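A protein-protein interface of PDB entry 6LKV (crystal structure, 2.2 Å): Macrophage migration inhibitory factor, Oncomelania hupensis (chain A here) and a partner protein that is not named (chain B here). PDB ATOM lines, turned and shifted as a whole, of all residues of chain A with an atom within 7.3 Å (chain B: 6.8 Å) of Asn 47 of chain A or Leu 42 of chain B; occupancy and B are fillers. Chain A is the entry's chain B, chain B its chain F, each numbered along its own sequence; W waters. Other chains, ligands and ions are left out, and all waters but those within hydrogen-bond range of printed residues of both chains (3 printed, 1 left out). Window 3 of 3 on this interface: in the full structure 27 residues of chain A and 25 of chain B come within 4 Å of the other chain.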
ATOM      1  N   THR A   8     -11.551  28.943 -24.199  1.00  0.00           N
ATOM      2  CA  THR A   8     -12.270  27.781 -24.785  1.00  0.00           C
ATOM      3  C   THR A   8     -11.272  26.740 -25.280  1.00  0.00           C
ATOM      4  O   THR A   8     -10.232  27.122 -25.852  1.00  0.00           O
ATOM      5  CB  THR A   8     -13.249  28.202 -25.886  1.00  0.00           C
ATOM      6  OG1 THR A   8     -13.975  27.021 -26.188  1.00  0.00           O
ATOM      7  CG2 THR A   8     -12.584  28.784 -27.111  1.00  0.00           C
ATOM      8  N   ASN A   9     -11.613  25.467 -25.056  1.00  0.00           N
ATOM      9  CA  ASN A   9     -10.856  24.311 -25.575  1.00  0.00           C
ATOM     10  C   ASN A   9     -11.224  24.104 -27.051  1.00  0.00           C
ATOM     11  O   ASN A   9     -10.558  23.316 -27.688  1.00  0.00           O
ATOM     12  CB  ASN A   9     -11.043  23.070 -24.696  1.00  0.00           C
ATOM     13  CG  ASN A   9     -12.484  22.652 -24.560  1.00  0.00           C
ATOM     14  OD1 ASN A   9     -13.392  23.384 -24.969  1.00  0.00           O
ATOM     15  ND2 ASN A   9     -12.690  21.471 -23.981  1.00  0.00           N
ATOM     16  N   ARG A  43      -8.728  33.101 -26.304  1.00  0.00           N
ATOM     17  CA  ARG A  43      -7.829  31.994 -25.930  1.00  0.00           C
ATOM     18  C   ARG A  43      -8.491  30.697 -26.380  1.00  0.00           C
ATOM     19  O   ARG A  43      -9.139  30.048 -25.562  1.00  0.00           O
ATOM     20  CB  ARG A  43      -7.531  32.081 -24.435  1.00  0.00           C
ATOM     21  CG  ARG A  43      -6.781  33.352 -24.112  1.00  0.00           C
ATOM     22  CD  ARG A  43      -7.580  34.254 -23.248  1.00  0.00           C
ATOM     23  NE  ARG A  43      -6.818  35.334 -22.664  1.00  0.00           N
ATOM     24  CZ  ARG A  43      -6.612  35.514 -21.363  1.00  0.00           C
ATOM     25  NH1 ARG A  43      -7.171  34.712 -20.464  1.00  0.00           N
ATOM     26  NH2 ARG A  43      -5.984  36.609 -20.980  1.00  0.00           N
ATOM     27  N   SER A  44      -8.335  30.361 -27.646  1.00  0.00           N
ATOM     28  CA  SER A  44      -8.859  29.111 -28.241  1.00  0.00           C
ATOM     29  C   SER A  44      -7.783  28.043 -28.104  1.00  0.00           C
ATOM     30  O   SER A  44      -6.622  28.401 -27.803  1.00  0.00           O
ATOM     31  CB  SER A  44      -9.306  29.350 -29.686  1.00  0.00           C
ATOM     32  OG  SER A  44      -8.216  29.640 -30.525  1.00  0.00           O
ATOM     33  N   GLY A  45      -8.158  26.776 -28.261  1.00  0.00           N
ATOM     34  CA  GLY A  45      -7.246  25.643 -28.041  1.00  0.00           C
ATOM     35  C   GLY A  45      -6.704  25.648 -26.624  1.00  0.00           C
ATOM     36  O   GLY A  45      -5.631  25.072 -26.399  1.00  0.00           O
ATOM     37  N   ALA A  46      -7.374  26.313 -25.686  1.00  0.00           N
ATOM     38  CA  ALA A  46      -6.887  26.424 -24.288  1.00  0.00           C
ATOM     39  C   ALA A  46      -6.970  25.050 -23.642  1.00  0.00           C
ATOM     40  O   ALA A  46      -7.910  24.294 -23.940  1.00  0.00           O
ATOM     41  CB  ALA A  46      -7.694  27.428 -23.482  1.00  0.00           C
ATOM     42  N   ASN A  47      -6.043  24.784 -22.743  1.00  0.00           N
ATOM     43  CA  ASN A  47      -6.079  23.606 -21.856  1.00  0.00           C
ATOM     44  C   ASN A  47      -7.040  23.912 -20.709  1.00  0.00           C
ATOM     45  O   ASN A  47      -6.592  24.031 -19.571  1.00  0.00           O
ATOM     46  CB  ASN A  47      -4.693  23.171 -21.398  1.00  0.00           C
ATOM     47  CG  ASN A  47      -4.756  21.810 -20.747  1.00  0.00           C
ATOM     48  OD1 ASN A  47      -5.824  21.173 -20.706  1.00  0.00           O
ATOM     49  ND2 ASN A  47      -3.640  21.372 -20.195  1.00  0.00           N
ATOM     50  N   ILE A  48      -8.324  23.982 -21.038  1.00  0.00           N
ATOM     51  CA  ILE A  48      -9.392  24.249 -20.056  1.00  0.00           C
ATOM     52  C   ILE A  48     -10.360  23.063 -20.107  1.00  0.00           C
ATOM     53  O   ILE A  48     -10.823  22.693 -21.193  1.00  0.00           O
ATOM     54  CB  ILE A  48     -10.044  25.620 -20.313  1.00  0.00           C
ATOM     55  CG1 ILE A  48     -11.012  25.948 -19.172  1.00  0.00           C
ATOM     56  CG2 ILE A  48     -10.694  25.698 -21.679  1.00  0.00           C
ATOM     57  CD1 ILE A  48     -11.453  27.380 -19.122  1.00  0.00           C
ATOM     58  N   MET A  49     -10.596  22.452 -18.962  1.00  0.00           N
ATOM     59  CA  MET A  49     -11.629  21.399 -18.789  1.00  0.00           C
ATOM     60  C   MET A  49     -12.699  21.918 -17.822  1.00  0.00           C
ATOM     61  O   MET A  49     -12.449  22.910 -17.093  1.00  0.00           O
ATOM     62  CB  MET A  49     -10.994  20.100 -18.259  1.00  0.00           C
ATOM     63  CG  MET A  49     -10.382  20.190 -16.894  1.00  0.00           C
ATOM     64  SD  MET A  49     -10.051  18.568 -16.083  1.00  0.00           S
ATOM     65  CE  MET A  49      -9.084  17.797 -17.381  1.00  0.00           C
ATOM     66  N   ARG A  54     -13.373  17.021 -20.976  1.00  0.00           N
ATOM     67  CA  ARG A  54     -12.786  17.869 -22.052  1.00  0.00           C
ATOM     68  C   ARG A  54     -13.764  18.033 -23.211  1.00  0.00           C
ATOM     69  O   ARG A  54     -13.338  18.410 -24.314  1.00  0.00           O
ATOM     70  CB  ARG A  54     -11.455  17.294 -22.542  1.00  0.00           C
ATOM     71  CG  ARG A  54     -10.407  17.165 -21.450  1.00  0.00           C
ATOM     72  CD  ARG A  54      -9.043  16.862 -22.011  1.00  0.00           C
ATOM     73  NE  ARG A  54      -7.999  16.959 -20.995  1.00  0.00           N
ATOM     74  CZ  ARG A  54      -7.337  18.068 -20.676  1.00  0.00           C
ATOM     75  NH1 ARG A  54      -7.604  19.212 -21.293  1.00  0.00           N
ATOM     76  NH2 ARG A  54      -6.387  18.032 -19.759  1.00  0.00           N
ATOM     77  N   ILE B   4     -10.552  27.563 -11.475  1.00  0.00           N
ATOM     78  CA  ILE B   4      -9.151  27.495 -10.995  1.00  0.00           C
ATOM     79  C   ILE B   4      -8.278  27.752 -12.218  1.00  0.00           C
ATOM     80  O   ILE B   4      -8.346  26.939 -13.190  1.00  0.00           O
ATOM     81  CB  ILE B   4      -8.843  26.132 -10.365  1.00  0.00           C
ATOM     82  CG1 ILE B   4     -10.022  25.553  -9.572  1.00  0.00           C
ATOM     83  CG2 ILE B   4      -7.565  26.205  -9.541  1.00  0.00           C
ATOM     84  CD1 ILE B   4     -10.498  26.416  -8.423  1.00  0.00           C
ATOM     85  N   THR B   5      -7.502  28.830 -12.201  1.00  0.00           N
ATOM     86  CA  THR B   5      -6.554  29.166 -13.291  1.00  0.00           C
ATOM     87  C   THR B   5      -5.151  28.935 -12.745  1.00  0.00           C
ATOM     88  O   THR B   5      -4.820  29.507 -11.683  1.00  0.00           O
ATOM     89  CB  THR B   5      -6.792  30.583 -13.825  1.00  0.00           C
ATOM     90  OG1 THR B   5      -8.175  30.708 -14.159  1.00  0.00           O
ATOM     91  CG2 THR B   5      -5.981  30.893 -15.055  1.00  0.00           C
ATOM     92  N   VAL B   6      -4.349  28.143 -13.461  1.00  0.00           N
ATOM     93  CA  VAL B   6      -2.947  27.888 -13.071  1.00  0.00           C
ATOM     94  C   VAL B   6      -2.047  28.454 -14.162  1.00  0.00           C
ATOM     95  O   VAL B   6      -2.128  27.974 -15.298  1.00  0.00           O
ATOM     96  CB  VAL B   6      -2.711  26.387 -12.838  1.00  0.00           C
ATOM     97  CG1 VAL B   6      -1.274  26.107 -12.435  1.00  0.00           C
ATOM     98  CG2 VAL B   6      -3.675  25.830 -11.791  1.00  0.00           C
ATOM     99  N   ASN B   7      -1.255  29.468 -13.816  1.00  0.00           N
ATOM    100  CA  ASN B   7      -0.271  30.114 -14.703  1.00  0.00           C
ATOM    101  C   ASN B   7       1.094  29.631 -14.229  1.00  0.00           C
ATOM    102  O   ASN B   7       1.464  29.980 -13.074  1.00  0.00           O
ATOM    103  CB  ASN B   7      -0.345  31.637 -14.668  1.00  0.00           C
ATOM    104  CG  ASN B   7      -1.736  32.145 -15.005  1.00  0.00           C
ATOM    105  OD1 ASN B   7      -2.114  32.159 -16.174  1.00  0.00           O
ATOM    106  ND2 ASN B   7      -2.500  32.523 -13.983  1.00  0.00           N
ATOM    107  N   THR B   8       1.790  28.840 -15.037  1.00  0.00           N
ATOM    108  CA  THR B   8       3.093  28.250 -14.643  1.00  0.00           C
ATOM    109  C   THR B   8       4.014  28.180 -15.848  1.00  0.00           C
ATOM    110  O   THR B   8       3.530  27.856 -16.962  1.00  0.00           O
ATOM    111  CB  THR B   8       2.953  26.877 -13.968  1.00  0.00           C
ATOM    112  OG1 THR B   8       4.250  26.497 -13.515  1.00  0.00           O
ATOM    113  CG2 THR B   8       2.399  25.803 -14.879  1.00  0.00           C
ATOM    114  N   VAL B  10       6.302  26.016 -15.873  1.00  0.00           N
ATOM    115  CA  VAL B  10       6.575  24.562 -16.033  1.00  0.00           C
ATOM    116  C   VAL B  10       5.954  24.097 -17.348  1.00  0.00           C
ATOM    117  O   VAL B  10       4.782  24.432 -17.628  1.00  0.00           O
ATOM    118  CB  VAL B  10       6.090  23.743 -14.826  1.00  0.00           C
ATOM    119  CG1 VAL B  10       6.204  22.252 -15.085  1.00  0.00           C
ATOM    120  CG2 VAL B  10       6.886  24.130 -13.577  1.00  0.00           C
ATOM    121  N   GLU B  12       4.284  22.035 -20.358  1.00  0.00           N
ATOM    122  CA  GLU B  12       3.130  21.108 -20.452  1.00  0.00           C
ATOM    123  C   GLU B  12       3.606  19.648 -20.364  1.00  0.00           C
ATOM    124  O   GLU B  12       2.979  18.871 -19.600  1.00  0.00           O
ATOM    125  CB  GLU B  12       2.359  21.335 -21.749  1.00  0.00           C
ATOM    126  CG  GLU B  12       1.061  20.568 -21.796  1.00  0.00           C
ATOM    127  CD  GLU B  12       0.192  20.943 -22.982  1.00  0.00           C
ATOM    128  OE1 GLU B  12      -0.489  21.974 -22.904  1.00  0.00           O
ATOM    129  OE2 GLU B  12       0.247  20.241 -23.987  1.00  0.00           O
ATOM    130  N   ILE B  15       4.118  17.915 -16.942  1.00  0.00           N
ATOM    131  CA  ILE B  15       3.004  17.935 -15.946  1.00  0.00           C
ATOM    132  C   ILE B  15       2.253  16.616 -16.044  1.00  0.00           C
ATOM    133  O   ILE B  15       1.806  16.245 -17.109  1.00  0.00           O
ATOM    134  CB  ILE B  15       2.084  19.151 -16.158  1.00  0.00           C
ATOM    135  CG1 ILE B  15       2.850  20.450 -15.898  1.00  0.00           C
ATOM    136  CG2 ILE B  15       0.851  19.039 -15.267  1.00  0.00           C
ATOM    137  CD1 ILE B  15       2.113  21.693 -16.301  1.00  0.00           C
ATOM    138  N   PRO B  16       2.040  15.891 -14.924  1.00  0.00           N
ATOM    139  CA  PRO B  16       1.252  14.664 -14.967  1.00  0.00           C
ATOM    140  C   PRO B  16      -0.103  14.918 -15.634  1.00  0.00           C
ATOM    141  O   PRO B  16      -0.697  15.941 -15.371  1.00  0.00           O
ATOM    142  CB  PRO B  16       1.084  14.288 -13.495  1.00  0.00           C
ATOM    143  CG  PRO B  16       2.293  14.929 -12.812  1.00  0.00           C
ATOM    144  CD  PRO B  16       2.540  16.212 -13.576  1.00  0.00           C
ATOM    145  N   PHE B  19      -3.239  15.928 -13.534  1.00  0.00           N
ATOM    146  CA  PHE B  19      -3.104  17.122 -12.662  1.00  0.00           C
ATOM    147  C   PHE B  19      -4.422  17.899 -12.631  1.00  0.00           C
ATOM    148  O   PHE B  19      -4.916  18.160 -11.515  1.00  0.00           O
ATOM    149  CB  PHE B  19      -1.936  18.008 -13.082  1.00  0.00           C
ATOM    150  CG  PHE B  19      -1.874  19.339 -12.376  1.00  0.00           C
ATOM    151  CD1 PHE B  19      -1.727  19.447 -11.001  1.00  0.00           C
ATOM    152  CD2 PHE B  19      -2.064  20.500 -13.096  1.00  0.00           C
ATOM    153  CE1 PHE B  19      -1.696  20.678 -10.381  1.00  0.00           C
ATOM    154  CE2 PHE B  19      -1.930  21.740 -12.491  1.00  0.00           C
ATOM    155  CZ  PHE B  19      -1.765  21.828 -11.132  1.00  0.00           C
ATOM    156  N   GLN B  20      -4.995  18.227 -13.790  1.00  0.00           N
ATOM    157  CA  GLN B  20      -6.257  19.013 -13.836  1.00  0.00           C
ATOM    158  C   GLN B  20      -7.414  18.237 -13.185  1.00  0.00           C
ATOM    159  O   GLN B  20      -8.187  18.844 -12.411  1.00  0.00           O
ATOM    160  CB  GLN B  20      -6.570  19.431 -15.257  1.00  0.00           C
ATOM    161  CG  GLN B  20      -5.655  20.553 -15.762  1.00  0.00           C
ATOM    162  CD  GLN B  20      -5.762  20.630 -17.261  1.00  0.00           C
ATOM    163  OE1 GLN B  20      -5.149  19.829 -17.955  1.00  0.00           O
ATOM    164  NE2 GLN B  20      -6.557  21.570 -17.762  1.00  0.00           N
ATOM    165  N   VAL B  40     -10.946  23.964 -14.605  1.00  0.00           N
ATOM    166  CA  VAL B  40      -9.486  24.120 -14.384  1.00  0.00           C
ATOM    167  C   VAL B  40      -8.841  24.504 -15.714  1.00  0.00           C
ATOM    168  O   VAL B  40      -8.888  23.715 -16.688  1.00  0.00           O
ATOM    169  CB  VAL B  40      -8.840  22.875 -13.767  1.00  0.00           C
ATOM    170  CG1 VAL B  40      -7.362  23.125 -13.501  1.00  0.00           C
ATOM    171  CG2 VAL B  40      -9.560  22.448 -12.495  1.00  0.00           C
ATOM    172  N   ASP B  41      -8.324  25.733 -15.752  1.00  0.00           N
ATOM    173  CA  ASP B  41      -7.655  26.332 -16.927  1.00  0.00           C
ATOM    174  C   ASP B  41      -6.156  26.328 -16.643  1.00  0.00           C
ATOM    175  O   ASP B  41      -5.712  27.118 -15.822  1.00  0.00           O
ATOM    176  CB  ASP B  41      -8.212  27.725 -17.190  1.00  0.00           C
ATOM    177  CG  ASP B  41      -7.704  28.379 -18.459  1.00  0.00           C
ATOM    178  OD1 ASP B  41      -6.858  27.782 -19.163  1.00  0.00           O
ATOM    179  OD2 ASP B  41      -8.161  29.491 -18.714  1.00  0.00           O
ATOM    180  N   LEU B  42      -5.429  25.404 -17.269  1.00  0.00           N
ATOM    181  CA  LEU B  42      -3.971  25.242 -17.075  1.00  0.00           C
ATOM    182  C   LEU B  42      -3.252  25.996 -18.203  1.00  0.00           C
ATOM    183  O   LEU B  42      -3.359  25.598 -19.374  1.00  0.00           O
ATOM    184  CB  LEU B  42      -3.621  23.753 -17.050  1.00  0.00           C
ATOM    185  CG  LEU B  42      -2.136  23.444 -16.981  1.00  0.00           C
ATOM    186  CD1 LEU B  42      -1.510  24.050 -15.718  1.00  0.00           C
ATOM    187  CD2 LEU B  42      -1.879  21.949 -17.085  1.00  0.00           C
ATOM    188  N   ARG B  43      -2.568  27.066 -17.849  1.00  0.00           N
ATOM    189  CA  ARG B  43      -1.639  27.785 -18.756  1.00  0.00           C
ATOM    190  C   ARG B  43      -0.221  27.358 -18.392  1.00  0.00           C
ATOM    191  O   ARG B  43       0.455  28.048 -17.597  1.00  0.00           O
ATOM    192  CB  ARG B  43      -1.890  29.294 -18.687  1.00  0.00           C
ATOM    193  CG  ARG B  43      -3.378  29.576 -18.788  1.00  0.00           C
ATOM    194  CD  ARG B  43      -3.634  31.009 -18.990  1.00  0.00           C
ATOM    195  NE  ARG B  43      -5.079  31.239 -18.957  1.00  0.00           N
ATOM    196  CZ  ARG B  43      -5.665  32.158 -18.243  1.00  0.00           C
ATOM    197  NH1 ARG B  43      -4.941  32.920 -17.432  1.00  0.00           N
ATOM    198  NH2 ARG B  43      -6.952  32.367 -18.413  1.00  0.00           N
ATOM    199  N   SER B  44       0.193  26.228 -18.962  1.00  0.00           N
ATOM    200  CA  SER B  44       1.552  25.674 -18.732  1.00  0.00           C
ATOM    201  C   SER B  44       2.446  26.229 -19.834  1.00  0.00           C
ATOM    202  O   SER B  44       1.888  26.802 -20.826  1.00  0.00           O
ATOM    203  CB  SER B  44       1.522  24.173 -18.670  1.00  0.00           C
ATOM    204  OG  SER B  44       1.117  23.592 -19.893  1.00  0.00           O
ATOM    205  N   LEU B  88       4.098  19.921 -10.071  1.00  0.00           N
ATOM    206  CA  LEU B  88       4.822  20.907 -10.913  1.00  0.00           C
ATOM    207  C   LEU B  88       6.276  21.028 -10.456  1.00  0.00           C
ATOM    208  O   LEU B  88       7.069  21.674 -11.193  1.00  0.00           O
ATOM    209  CB  LEU B  88       4.117  22.270 -10.876  1.00  0.00           C
ATOM    210  CG  LEU B  88       2.610  22.232 -11.125  1.00  0.00           C
ATOM    211  CD1 LEU B  88       2.015  23.624 -11.130  1.00  0.00           C
ATOM    212  CD2 LEU B  88       2.311  21.503 -12.427  1.00  0.00           C
HETATM  213  O   HOH W   1      -7.040  35.560 -18.081  1.00  0.00           O
HETATM  214  O   HOH W   2      -1.426  22.851 -20.766  1.00  0.00           O
HETATM  215  O   HOH W   3      -5.082  26.982 -20.914  1.00  0.00           O
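Water W2 lies within hydrogen-bond range of the side-chain carboxylate (OE1) of Glu 12 of chain B, the side-chain amide nitrogen (ND2) of Asn 47 of chain A and the side-chain hydroxyl (OG) of Ser 44 of chain B.
Water W1 bridges the guanidinium group (NH1) of Arg 43 of chain A (2.5 Å) and the guanidinium group (NH2) of Arg 43 of chain B (3.2 Å).
Water W3 lies within hydrogen-bond range of OD1 of Asp 41 of chain B (2.6 Å), O of Leu 42 of chain B (2.7 Å) and N of Asn 47 of chain A (3.0 Å).
Among the printed residues, merely in contact across the chains: Ile 48 of chain A with Val 40 of chain B (3.4 Å), Asn 47 of chain A with Asp 41 of chain B (3.7 Å), Met 49 of chain A with Gln 20 of chain B (3.7 Å), Asn 47 of chain A with Val 40 of chain B (3.7 Å) and Ile 48 of chain A with Asp 41 of chain B (3.8 Å).
The backbone NH of Leu 42 of chain B lies within hydrogen-bond range of the backbone carbonyl oxygen of Asn 47 of chain A.
NH2 of Arg 43 of chain B lies close to NH1 of Arg 43 of chain A, at 3.1 Å.
NE2 of Gln 20 of chain B sits at hydrogen-bond distance from O of Asn 47 of chain A (3.1 Å).
NH2 of Arg 54 of chain A lies within hydrogen-bond range of OE1 of Gln 20 of chain B (2.8 Å).
O of Met 49 of chain A sits at hydrogen-bond distance from N of Val 40 of chain B (3.1 Å).
Printed residues of chain B within 4 Å of Arg 43 of chain A: Arg 43 (3.1 Å).
Printed residues of chain B within 4 Å of Ile 48 of chain A: Val 40 (3.4 Å) and Asp 41 (3.8 Å).
Of the printed residues of chain B, Met 49 of chain A touches Gln 20 and Val 40.
Thr 5 of chain B touches none of the printed residues of chain A.
Of the printed residues of chain A, Gln 20 of chain B touches Asn 47 (3.1 Å), Met 49 (3.7 Å) and Arg 54 (2.8 Å).
Of the printed residues of chain A, Val 40 of chain B touches Asn 47, Ile 48 and Met 49.
The nearest residue of chain B that does not touch Asn 47 of chain A is Glu 12 of chain B (4.2 Å).
The nearest residue of chain A that does not touch Leu 42 of chain B is Ile 48 of chain A (5.0 Å).
Hydrophobic or aromatic side chains of chain B that line the printed part of chain A: Leu 42.
Along chain B the printed residues that touch a printed residue of chain A span positions 20 to 43.
Of the 10 printed residues of chain A, 5 touch a printed residue of chain B.
Hydrophobic or aromatic side chains of chain A that line the printed part of chain B: Ile 48 and Met 49.
Along chain A the printed residues that touch a printed residue of chain B span positions 43 to 54.
Among the printed residues, no Asp or Glu carboxylate lies within 4 Å of a Lys or Arg side-chain nitrogen of the other chain.
O of Val 6 of chain B lies within hydrogen-bond range of N of Arg 43 of chain B, at 2.7 Å.
The backbone carbonyl oxygen (O) of Arg 54 of chain A sits at hydrogen-bond distance from the side-chain amide nitrogen (ND2) of Asn 9 of chain A, at 3.1 Å.
OD1 of Asn 47 of chain A lies within hydrogen-bond range of NH1 of Arg 54 of chain A (2.7 Å).
The backbone carbonyl oxygen (O) of Arg 43 of chain A sits at hydrogen-bond distance from the backbone NH (N) of Thr 8 of chain A, at 3.0 Å.
OD1 of Asn 7 of chain B is in hydrogen-bond range of NH1 of Arg 43 of chain B (3.2 Å).
The side-chain carboxylate of Asp 41 of chain B lies within salt-bridge range of the guanidinium group of Arg 43 of chain B (3.1 Å).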
